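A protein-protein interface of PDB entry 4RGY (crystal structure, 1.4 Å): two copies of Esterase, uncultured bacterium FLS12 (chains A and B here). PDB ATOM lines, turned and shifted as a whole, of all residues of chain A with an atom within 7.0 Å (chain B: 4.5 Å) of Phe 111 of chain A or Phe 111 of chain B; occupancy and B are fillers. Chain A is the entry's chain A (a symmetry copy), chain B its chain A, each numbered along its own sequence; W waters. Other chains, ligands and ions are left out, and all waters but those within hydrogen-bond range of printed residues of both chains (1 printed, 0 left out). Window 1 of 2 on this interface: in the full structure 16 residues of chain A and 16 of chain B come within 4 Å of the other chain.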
ATOM      1  N   LEU A   4     -16.829  16.068  28.860  1.00  0.00           N
ATOM      2  CA  LEU A   4     -15.573  15.863  29.575  1.00  0.00           C
ATOM      3  C   LEU A   4     -14.391  15.911  28.615  1.00  0.00           C
ATOM      4  O   LEU A   4     -14.409  15.263  27.569  1.00  0.00           O
ATOM      5  CB  LEU A   4     -15.610  14.503  30.282  1.00  0.00           C
ATOM      6  CG  LEU A   4     -14.321  14.035  30.963  1.00  0.00           C
ATOM      7  CD1 LEU A   4     -14.020  14.888  32.161  1.00  0.00           C
ATOM      8  CD2 LEU A   4     -14.416  12.573  31.373  1.00  0.00           C
ATOM      9  N   PHE A   5     -13.372  16.688  28.966  1.00  0.00           N
ATOM     10  CA  PHE A   5     -12.207  16.820  28.107  1.00  0.00           C
ATOM     11  C   PHE A   5     -10.957  16.474  28.872  1.00  0.00           C
ATOM     12  O   PHE A   5     -10.666  17.066  29.918  1.00  0.00           O
ATOM     13  CB  PHE A   5     -12.089  18.253  27.575  1.00  0.00           C
ATOM     14  CG  PHE A   5     -13.291  18.703  26.819  1.00  0.00           C
ATOM     15  CD1 PHE A   5     -14.376  19.247  27.481  1.00  0.00           C
ATOM     16  CD2 PHE A   5     -13.349  18.571  25.441  1.00  0.00           C
ATOM     17  CE1 PHE A   5     -15.508  19.643  26.783  1.00  0.00           C
ATOM     18  CE2 PHE A   5     -14.470  18.974  24.737  1.00  0.00           C
ATOM     19  CZ  PHE A   5     -15.556  19.509  25.408  1.00  0.00           C
ATOM     20  N   GLN A   6     -10.200  15.519  28.345  1.00  0.00           N
ATOM     21  CA  GLN A   6      -8.854  15.282  28.822  1.00  0.00           C
ATOM     22  C   GLN A   6      -7.928  15.983  27.837  1.00  0.00           C
ATOM     23  O   GLN A   6      -7.922  15.681  26.642  1.00  0.00           O
ATOM     24  CB  GLN A   6      -8.567  13.787  28.909  1.00  0.00           C
ATOM     25  CG  GLN A   6      -9.495  13.049  29.890  1.00  0.00           C
ATOM     26  CD  GLN A   6      -9.300  13.435  31.355  1.00  0.00           C
ATOM     27  OE1 GLN A   6      -8.324  14.088  31.725  1.00  0.00           O
ATOM     28  NE2 GLN A   6     -10.241  13.020  32.198  1.00  0.00           N
ATOM     29  N   CYS A   7      -7.177  16.949  28.344  1.00  0.00           N
ATOM     30  CA  CYS A   7      -6.431  17.874  27.504  1.00  0.00           C
ATOM     31  C   CYS A   7      -4.948  17.700  27.721  1.00  0.00           C
ATOM     32  O   CYS A   7      -4.454  17.896  28.839  1.00  0.00           O
ATOM     33  CB  CYS A   7      -6.795  19.317  27.880  1.00  0.00           C
ATOM     34  SG  CYS A   7      -8.568  19.643  28.124  1.00  0.00           S
ATOM     35  N   MET A  20      -4.660  18.580  31.693  1.00  0.00           N
ATOM     36  CA  MET A  20      -5.713  19.019  32.604  1.00  0.00           C
ATOM     37  C   MET A  20      -7.018  18.335  32.225  1.00  0.00           C
ATOM     38  O   MET A  20      -7.177  17.829  31.104  1.00  0.00           O
ATOM     39  CB  MET A  20      -5.895  20.536  32.557  1.00  0.00           C
ATOM     40  CG  MET A  20      -6.410  21.061  31.231  1.00  0.00           C
ATOM     41  SD  MET A  20      -6.626  22.844  31.333  1.00  0.00           S
ATOM     42  CE  MET A  20      -6.751  23.260  29.597  1.00  0.00           C
ATOM     43  N   THR A  21      -7.960  18.307  33.168  1.00  0.00           N
ATOM     44  CA  THR A  21      -9.299  17.798  32.905  1.00  0.00           C
ATOM     45  C   THR A  21     -10.254  18.973  32.952  1.00  0.00           C
ATOM     46  O   THR A  21     -10.179  19.786  33.871  1.00  0.00           O
ATOM     47  CB  THR A  21      -9.712  16.800  33.992  1.00  0.00           C
ATOM     48  OG1 THR A  21      -8.740  15.746  34.056  1.00  0.00           O
ATOM     49  CG2 THR A  21     -11.085  16.221  33.710  1.00  0.00           C
ATOM     50  N   VAL A  22     -11.131  19.074  31.963  1.00  0.00           N
ATOM     51  CA  VAL A  22     -12.108  20.156  31.913  1.00  0.00           C
ATOM     52  C   VAL A  22     -13.499  19.572  31.730  1.00  0.00           C
ATOM     53  O   VAL A  22     -13.704  18.668  30.916  1.00  0.00           O
ATOM     54  CB  VAL A  22     -11.788  21.141  30.759  1.00  0.00           C
ATOM     55  CG1 VAL A  22     -12.915  22.137  30.554  1.00  0.00           C
ATOM     56  CG2 VAL A  22     -10.470  21.869  31.030  1.00  0.00           C
ATOM     57  N   ILE A  23     -14.467  20.078  32.492  1.00  0.00           N
ATOM     58  CA  ILE A  23     -15.853  19.744  32.193  1.00  0.00           C
ATOM     59  C   ILE A  23     -16.620  21.001  31.809  1.00  0.00           C
ATOM     60  O   ILE A  23     -16.480  22.047  32.451  1.00  0.00           O
ATOM     61  CB  ILE A  23     -16.546  18.968  33.321  1.00  0.00           C
ATOM     62  CG1 ILE A  23     -16.310  19.616  34.667  1.00  0.00           C
ATOM     63  CG2 ILE A  23     -16.043  17.532  33.366  1.00  0.00           C
ATOM     64  CD1 ILE A  23     -16.996  18.870  35.811  1.00  0.00           C
ATOM     65  N   LEU A  24     -17.386  20.887  30.725  1.00  0.00           N
ATOM     66  CA  LEU A  24     -18.112  22.007  30.133  1.00  0.00           C
ATOM     67  C   LEU A  24     -19.576  21.651  30.057  1.00  0.00           C
ATOM     68  O   LEU A  24     -19.919  20.528  29.694  1.00  0.00           O
ATOM     69  CB  LEU A  24     -17.673  22.222  28.686  1.00  0.00           C
ATOM     70  CG  LEU A  24     -16.552  23.122  28.209  1.00  0.00           C
ATOM     71  CD1 LEU A  24     -16.655  23.246  26.681  1.00  0.00           C
ATOM     72  CD2 LEU A  24     -16.617  24.490  28.879  1.00  0.00           C
ATOM     73  N   GLU A  42     -19.597  32.164  27.229  1.00  0.00           N
ATOM     74  CA  GLU A  42     -18.590  32.445  28.243  1.00  0.00           C
ATOM     75  C   GLU A  42     -19.048  31.932  29.597  1.00  0.00           C
ATOM     76  O   GLU A  42     -19.528  32.697  30.440  1.00  0.00           O
ATOM     77  CB  GLU A  42     -18.299  33.942  28.308  1.00  0.00           C
ATOM     78  CG  GLU A  42     -17.764  34.518  27.009  1.00  0.00           C
ATOM     79  CD  GLU A  42     -17.739  36.032  27.026  1.00  0.00           C
ATOM     80  OE1 GLU A  42     -18.742  36.649  26.607  1.00  0.00           O
ATOM     81  OE2 GLU A  42     -16.717  36.602  27.460  1.00  0.00           O
ATOM     82  N   ALA A  75     -18.537  25.731  34.260  1.00  0.00           N
ATOM     83  CA  ALA A  75     -17.421  24.928  33.768  1.00  0.00           C
ATOM     84  C   ALA A  75     -16.442  24.680  34.916  1.00  0.00           C
ATOM     85  O   ALA A  75     -16.343  25.486  35.846  1.00  0.00           O
ATOM     86  CB  ALA A  75     -16.734  25.626  32.619  1.00  0.00           C
ATOM     87  N   VAL A  77     -12.324  23.553  35.661  1.00  0.00           N
ATOM     88  CA  VAL A  77     -10.991  23.319  35.112  1.00  0.00           C
ATOM     89  C   VAL A  77     -10.111  22.746  36.209  1.00  0.00           C
ATOM     90  O   VAL A  77      -9.927  23.381  37.245  1.00  0.00           O
ATOM     91  CB  VAL A  77     -10.363  24.626  34.566  1.00  0.00           C
ATOM     92  CG1 VAL A  77      -8.911  24.404  34.130  1.00  0.00           C
ATOM     93  CG2 VAL A  77     -11.191  25.170  33.395  1.00  0.00           C
ATOM     94  N   LEU A 106      -4.766  29.661  28.879  1.00  0.00           N
ATOM     95  CA  LEU A 106      -4.870  28.513  27.983  1.00  0.00           C
ATOM     96  C   LEU A 106      -6.276  27.923  28.003  1.00  0.00           C
ATOM     97  O   LEU A 106      -6.852  27.605  26.961  1.00  0.00           O
ATOM     98  CB  LEU A 106      -3.844  27.442  28.355  1.00  0.00           C
ATOM     99  CG  LEU A 106      -2.388  27.762  27.998  1.00  0.00           C
ATOM    100  CD1 LEU A 106      -1.449  26.762  28.643  1.00  0.00           C
ATOM    101  CD2 LEU A 106      -2.170  27.795  26.488  1.00  0.00           C
ATOM    102  N   ALA A 107      -6.840  27.770  29.192  1.00  0.00           N
ATOM    103  CA  ALA A 107      -8.190  27.241  29.295  1.00  0.00           C
ATOM    104  C   ALA A 107      -9.180  28.116  28.536  1.00  0.00           C
ATOM    105  O   ALA A 107     -10.028  27.606  27.802  1.00  0.00           O
ATOM    106  CB  ALA A 107      -8.603  27.100  30.757  1.00  0.00           C
ATOM    107  N   ARG A 108      -9.049  29.430  28.687  1.00  0.00           N
ATOM    108  CA  ARG A 108      -9.942  30.368  28.015  1.00  0.00           C
ATOM    109  C   ARG A 108      -9.726  30.396  26.500  1.00  0.00           C
ATOM    110  O   ARG A 108     -10.652  30.692  25.743  1.00  0.00           O
ATOM    111  CB  ARG A 108      -9.770  31.765  28.620  1.00  0.00           C
ATOM    112  CG  ARG A 108     -10.398  31.888  29.997  1.00  0.00           C
ATOM    113  CD  ARG A 108      -9.851  33.079  30.768  1.00  0.00           C
ATOM    114  NE  ARG A 108     -10.497  33.177  32.074  1.00  0.00           N
ATOM    115  CZ  ARG A 108      -9.934  33.722  33.146  1.00  0.00           C
ATOM    116  NH1 ARG A 108      -8.708  34.218  33.073  1.00  0.00           N
ATOM    117  NH2 ARG A 108     -10.604  33.756  34.291  1.00  0.00           N
ATOM    118  N   SER A 109      -8.515  30.079  26.057  1.00  0.00           N
ATOM    119  CA  SER A 109      -8.221  30.027  24.627  1.00  0.00           C
ATOM    120  C   SER A 109      -8.825  28.772  23.981  1.00  0.00           C
ATOM    121  O   SER A 109      -9.255  28.806  22.826  1.00  0.00           O
ATOM    122  CB  SER A 109      -6.710  30.092  24.378  1.00  0.00           C
ATOM    123  OG  SER A 109      -6.086  28.826  24.544  1.00  0.00           O
ATOM    124  N   PHE A 110      -8.889  27.673  24.734  1.00  0.00           N
ATOM    125  CA  PHE A 110      -9.408  26.415  24.204  1.00  0.00           C
ATOM    126  C   PHE A 110     -10.936  26.337  24.266  1.00  0.00           C
ATOM    127  O   PHE A 110     -11.587  25.784  23.369  1.00  0.00           O
ATOM    128  CB  PHE A 110      -8.883  25.228  25.018  1.00  0.00           C
ATOM    129  CG  PHE A 110      -7.388  25.051  24.993  1.00  0.00           C
ATOM    130  CD1 PHE A 110      -6.611  25.525  23.946  1.00  0.00           C
ATOM    131  CD2 PHE A 110      -6.763  24.368  26.032  1.00  0.00           C
ATOM    132  CE1 PHE A 110      -5.229  25.333  23.949  1.00  0.00           C
ATOM    133  CE2 PHE A 110      -5.395  24.178  26.045  1.00  0.00           C
ATOM    134  CZ  PHE A 110      -4.624  24.661  25.007  1.00  0.00           C
ATOM    135  N   PHE A 111     -11.506  26.839  25.359  1.00  0.00           N
ATOM    136  CA  PHE A 111     -12.902  26.596  25.710  1.00  0.00           C
ATOM    137  C   PHE A 111     -13.676  27.900  25.874  1.00  0.00           C
ATOM    138  O   PHE A 111     -13.080  28.956  26.103  1.00  0.00           O
ATOM    139  CB  PHE A 111     -12.990  25.759  27.001  1.00  0.00           C
ATOM    140  CG  PHE A 111     -12.398  24.376  26.874  1.00  0.00           C
ATOM    141  CD1 PHE A 111     -13.026  23.409  26.094  1.00  0.00           C
ATOM    142  CD2 PHE A 111     -11.227  24.045  27.534  1.00  0.00           C
ATOM    143  CE1 PHE A 111     -12.485  22.138  25.976  1.00  0.00           C
ATOM    144  CE2 PHE A 111     -10.683  22.771  27.415  1.00  0.00           C
ATOM    145  CZ  PHE A 111     -11.323  21.819  26.636  1.00  0.00           C
ATOM    146  N   PRO A 112     -15.009  27.835  25.755  1.00  0.00           N
ATOM    147  CA  PRO A 112     -15.838  29.042  25.846  1.00  0.00           C
ATOM    148  C   PRO A 112     -16.064  29.439  27.303  1.00  0.00           C
ATOM    149  O   PRO A 112     -17.172  29.333  27.837  1.00  0.00           O
ATOM    150  CB  PRO A 112     -17.141  28.611  25.161  1.00  0.00           C
ATOM    151  CG  PRO A 112     -17.218  27.150  25.397  1.00  0.00           C
ATOM    152  CD  PRO A 112     -15.796  26.655  25.354  1.00  0.00           C
ATOM    153  N   LEU A 113     -14.983  29.898  27.928  1.00  0.00           N
ATOM    154  CA  LEU A 113     -14.978  30.240  29.343  1.00  0.00           C
ATOM    155  C   LEU A 113     -14.984  31.746  29.567  1.00  0.00           C
ATOM    156  O   LEU A 113     -14.359  32.502  28.817  1.00  0.00           O
ATOM    157  CB  LEU A 113     -13.742  29.639  30.010  1.00  0.00           C
ATOM    158  CG  LEU A 113     -13.505  28.142  29.797  1.00  0.00           C
ATOM    159  CD1 LEU A 113     -12.288  27.722  30.597  1.00  0.00           C
ATOM    160  CD2 LEU A 113     -14.708  27.317  30.193  1.00  0.00           C
ATOM    161  N   ALA A 114     -15.687  32.169  30.613  1.00  0.00           N
ATOM    162  CA  ALA A 114     -15.701  33.575  31.025  1.00  0.00           C
ATOM    163  C   ALA A 114     -14.328  34.064  31.461  1.00  0.00           C
ATOM    164  O   ALA A 114     -13.468  33.279  31.865  1.00  0.00           O
ATOM    165  CB  ALA A 114     -16.701  33.786  32.149  1.00  0.00           C
ATOM    166  N   PHE B   5      -7.133  16.839  22.532  1.00  0.00           N
ATOM    167  CA  PHE B   5      -8.297  16.707  23.390  1.00  0.00           C
ATOM    168  C   PHE B   5      -8.988  15.394  23.129  1.00  0.00           C
ATOM    169  O   PHE B   5      -9.378  15.095  21.995  1.00  0.00           O
ATOM    170  CB  PHE B   5      -9.284  17.852  23.141  1.00  0.00           C
ATOM    171  CG  PHE B   5      -8.689  19.201  23.351  1.00  0.00           C
ATOM    172  CD1 PHE B   5      -8.000  19.834  22.331  1.00  0.00           C
ATOM    173  CD2 PHE B   5      -8.802  19.841  24.574  1.00  0.00           C
ATOM    174  CE1 PHE B   5      -7.422  21.078  22.531  1.00  0.00           C
ATOM    175  CE2 PHE B   5      -8.237  21.088  24.778  1.00  0.00           C
ATOM    176  CZ  PHE B   5      -7.542  21.710  23.755  1.00  0.00           C
ATOM    177  N   CYS B   7     -12.411  13.859  23.980  1.00  0.00           N
ATOM    178  CA  CYS B   7     -13.676  14.475  24.351  1.00  0.00           C
ATOM    179  C   CYS B   7     -14.745  13.422  24.507  1.00  0.00           C
ATOM    180  O   CYS B   7     -15.066  12.712  23.545  1.00  0.00           O
ATOM    181  CB  CYS B   7     -14.123  15.440  23.244  1.00  0.00           C
ATOM    182  SG  CYS B   7     -12.826  16.522  22.573  1.00  0.00           S
ATOM    183  N   VAL B  22      -9.776  15.648  19.172  1.00  0.00           N
ATOM    184  CA  VAL B  22      -9.597  16.932  18.504  1.00  0.00           C
ATOM    185  C   VAL B  22      -8.172  17.418  18.717  1.00  0.00           C
ATOM    186  O   VAL B  22      -7.639  17.347  19.826  1.00  0.00           O
ATOM    187  CB  VAL B  22     -10.603  17.983  19.040  1.00  0.00           C
ATOM    188  CG1 VAL B  22     -10.280  19.373  18.521  1.00  0.00           C
ATOM    189  CG2 VAL B  22     -12.034  17.589  18.668  1.00  0.00           C
ATOM    190  N   LEU B  24      -5.924  20.964  18.247  1.00  0.00           N
ATOM    191  CA  LEU B  24      -6.062  22.405  18.061  1.00  0.00           C
ATOM    192  C   LEU B  24      -4.688  23.027  18.056  1.00  0.00           C
ATOM    193  O   LEU B  24      -3.843  22.662  18.871  1.00  0.00           O
ATOM    194  CB  LEU B  24      -6.784  23.030  19.253  1.00  0.00           C
ATOM    195  CG  LEU B  24      -8.278  23.235  19.394  1.00  0.00           C
ATOM    196  CD1 LEU B  24      -8.523  24.144  20.609  1.00  0.00           C
ATOM    197  CD2 LEU B  24      -8.877  23.836  18.127  1.00  0.00           C
ATOM    198  N   ALA B 107     -18.591  20.372  17.869  1.00  0.00           N
ATOM    199  CA  ALA B 107     -17.183  20.726  17.819  1.00  0.00           C
ATOM    200  C   ALA B 107     -16.998  22.239  17.854  1.00  0.00           C
ATOM    201  O   ALA B 107     -16.149  22.747  18.589  1.00  0.00           O
ATOM    202  CB  ALA B 107     -16.520  20.128  16.583  1.00  0.00           C
ATOM    203  N   ARG B 108     -17.813  22.954  17.087  1.00  0.00           N
ATOM    204  CA  ARG B 108     -17.726  24.410  17.032  1.00  0.00           C
ATOM    205  C   ARG B 108     -18.175  25.071  18.339  1.00  0.00           C
ATOM    206  O   ARG B 108     -17.718  26.165  18.674  1.00  0.00           O
ATOM    207  CB  ARG B 108     -18.545  24.929  15.845  1.00  0.00           C
ATOM    208  CG  ARG B 108     -17.871  24.668  14.511  1.00  0.00           C
ATOM    209  CD  ARG B 108     -18.849  24.758  13.351  1.00  0.00           C
ATOM    210  NE  ARG B 108     -18.158  24.527  12.086  1.00  0.00           N
ATOM    211  CZ  ARG B 108     -18.737  24.031  10.999  1.00  0.00           C
ATOM    212  NH1 ARG B 108     -20.022  23.709  11.019  1.00  0.00           N
ATOM    213  NH2 ARG B 108     -18.019  23.851   9.897  1.00  0.00           N
ATOM    214  N   SER B 109     -19.055  24.407  19.079  1.00  0.00           N
ATOM    215  CA  SER B 109     -19.508  24.929  20.367  1.00  0.00           C
ATOM    216  C   SER B 109     -18.425  24.765  21.443  1.00  0.00           C
ATOM    217  O   SER B 109     -18.291  25.609  22.332  1.00  0.00           O
ATOM    218  CB  SER B 109     -20.812  24.252  20.801  1.00  0.00           C
ATOM    219  OG  SER B 109     -20.583  22.986  21.404  1.00  0.00           O
ATOM    220  N   PHE B 110     -17.631  23.698  21.347  1.00  0.00           N
ATOM    221  CA  PHE B 110     -16.596  23.426  22.342  1.00  0.00           C
ATOM    222  C   PHE B 110     -15.302  24.198  22.070  1.00  0.00           C
ATOM    223  O   PHE B 110     -14.617  24.649  22.997  1.00  0.00           O
ATOM    224  CB  PHE B 110     -16.221  21.941  22.339  1.00  0.00           C
ATOM    225  CG  PHE B 110     -17.339  21.001  22.703  1.00  0.00           C
ATOM    226  CD1 PHE B 110     -18.412  21.406  23.484  1.00  0.00           C
ATOM    227  CD2 PHE B 110     -17.288  19.679  22.273  1.00  0.00           C
ATOM    228  CE1 PHE B 110     -19.425  20.505  23.812  1.00  0.00           C
ATOM    229  CE2 PHE B 110     -18.290  18.782  22.590  1.00  0.00           C
ATOM    230  CZ  PHE B 110     -19.362  19.191  23.356  1.00  0.00           C
ATOM    231  N   PHE B 111     -14.935  24.297  20.793  1.00  0.00           N
ATOM    232  CA  PHE B 111     -13.607  24.741  20.382  1.00  0.00           C
ATOM    233  C   PHE B 111     -13.679  25.950  19.455  1.00  0.00           C
ATOM    234  O   PHE B 111     -14.715  26.198  18.830  1.00  0.00           O
ATOM    235  CB  PHE B 111     -12.848  23.589  19.695  1.00  0.00           C
ATOM    236  CG  PHE B 111     -12.576  22.411  20.600  1.00  0.00           C
ATOM    237  CD1 PHE B 111     -11.659  22.518  21.640  1.00  0.00           C
ATOM    238  CD2 PHE B 111     -13.230  21.206  20.405  1.00  0.00           C
ATOM    239  CE1 PHE B 111     -11.407  21.438  22.471  1.00  0.00           C
ATOM    240  CE2 PHE B 111     -12.979  20.122  21.240  1.00  0.00           C
ATOM    241  CZ  PHE B 111     -12.060  20.245  22.271  1.00  0.00           C
ATOM    242  N   PRO B 112     -12.582  26.713  19.362  1.00  0.00           N
ATOM    243  CA  PRO B 112     -12.569  27.926  18.537  1.00  0.00           C
ATOM    244  C   PRO B 112     -12.361  27.580  17.064  1.00  0.00           C
ATOM    245  O   PRO B 112     -11.311  27.861  16.477  1.00  0.00           O
ATOM    246  CB  PRO B 112     -11.387  28.716  19.113  1.00  0.00           C
ATOM    247  CG  PRO B 112     -10.467  27.677  19.635  1.00  0.00           C
ATOM    248  CD  PRO B 112     -11.352  26.577  20.162  1.00  0.00           C
ATOM    249  N   LEU B 113     -13.388  26.963  16.488  1.00  0.00           N
ATOM    250  CA  LEU B 113     -13.343  26.473  15.117  1.00  0.00           C
ATOM    251  C   LEU B 113     -14.142  27.355  14.168  1.00  0.00           C
ATOM    252  O   LEU B 113     -15.199  27.882  14.529  1.00  0.00           O
ATOM    253  CB  LEU B 113     -13.897  25.051  15.065  1.00  0.00           C
ATOM    254  CG  LEU B 113     -13.288  24.039  16.039  1.00  0.00           C
ATOM    255  CD1 LEU B 113     -13.905  22.679  15.779  1.00  0.00           C
ATOM    256  CD2 LEU B 113     -11.783  23.969  15.915  1.00  0.00           C
HETATM  257  O   HOH W   1     -13.866  27.477  22.492  1.00  0.00           O
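The backbone carbonyl oxygen (O) of Phe 110 of chain A lies close to the backbone carbonyl oxygen (O) of Phe 110 of chain B.
O of Phe 5 of chain B is in hydrogen-bond range of SG of Cys 7 of chain B.
O of Val 22 of chain B is in hydrogen-bond range of N of Phe 5 of chain B, 2.8 Å away.
The backbone carbonyl oxygen of Phe 5 of chain A is in hydrogen-bond range of the side-chain sulfur of Cys 7 of chain A (3.8 Å).
The backbone NH of Phe 5 of chain A sits at hydrogen-bond distance from the backbone carbonyl oxygen of Val 22 of chain A, at 2.8 Å.
OE1 of Gln 6 of chain A sits at hydrogen-bond distance from OG1 of Thr 21 of chain A (2.9 Å).
The side-chain hydroxyl of Ser 109 of chain A lies within hydrogen-bond range of the backbone carbonyl oxygen of Leu 106 of chain A (2.8 Å).
Among the printed residues, merely in contact across the chains: Leu 4 of chain A with Cys 7 of chain B, Phe 5 of chain A with Cys 7 of chain B, Phe 5 of chain A with Phe 110 of chain B, Phe 5 of chain A with Phe 111 of chain B, Gln 6 of chain A with Phe 5 of chain B, Cys 7 of chain A with Phe 5 of chain B, Ser 109 of chain A with Pro 112 of chain B, Phe 110 of chain A with Phe 5 of chain B, Phe 110 of chain A with Phe 111 of chain B, Phe 110 of chain A with Pro 112 of chain B, Phe 111 of chain A with Phe 5 of chain B, Phe 111 of chain A with Phe 110 of chain B, Phe 111 of chain A with Phe 111 of chain B, Pro 112 of chain A with Ser 109 of chain B and Pro 112 of chain A with Phe 110 of chain B.
Of the printed residues of chain B, Leu 4 of chain A touches Cys 7 (3.4 Å).
Printed residues of chain B within 4 Å of Gln 6 of chain A: Phe 5 (3.4 Å).
Glu 42 of chain A touches none of the printed residues of chain B.
Val 77 of chain A touches none of the printed residues of chain B.
Printed residues of chain B within 4 Å of Ser 109 of chain A: Pro 112.
Of the printed residues of chain B, Phe 110 of chain A touches Phe 5 (3.6 Å), Phe 110 (3.3 Å), Phe 111 (3.7 Å) and Pro 112 (3.3 Å).
Of chain B, only Phe 5, Phe 110 and Phe 111 come within 4 Å of Phe 111 of chain A.
Of the printed residues of chain A, Cys 7 of chain B touches Leu 4 (3.4 Å) and Phe 5 (3.6 Å).
Of chain A, only Phe 5, Phe 110 and Phe 111 come within 4 Å of Phe 111 of chain B.
The nearest printed residue of chain B that does not touch Phe 111 of chain A is Pro 112 of chain B (5.2 Å).
The nearest printed residue of chain A that does not touch Phe 5 of chain B is Phe 5 of chain A (4.7 Å).
Printed residues of chain B that touch a printed residue of chain A: Phe 5, Cys 7, Ser 109, Phe 110, Phe 111 and Pro 112.
Hydrophobic or aromatic side chains of chain B that line the printed part of chain A: Phe 5, Phe 110, Phe 111 and Pro 112.
Hydrophobic or aromatic side chains of chain A within 4 Å of the printed part of chain B: Phe 5, Phe 110, Phe 111 and Pro 112.
Among the printed residues, 16 pairs touch across the chains.
Phe 5 of chain A touches Phe 111 of chain B, and with the chains exchanged Phe 111 of chain A touches Phe 5 of chain B.
Phe 110 of chain B touches its own counterpart, Phe 110 of chain A.
Phe 110 of chain A touches Pro 112 of chain B, and with the chains exchanged Pro 112 of chain A touches Phe 110 of chain B.
Phe 111 of chain A touches its own counterpart, Phe 111 of chain B.
Water W1 lies within hydrogen-bond range of the backbone carbonyl oxygen (O) of Phe 110 of chain B (3.0 Å) and the backbone carbonyl oxygen (O) of Phe 110 of chain A (3.0 Å).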
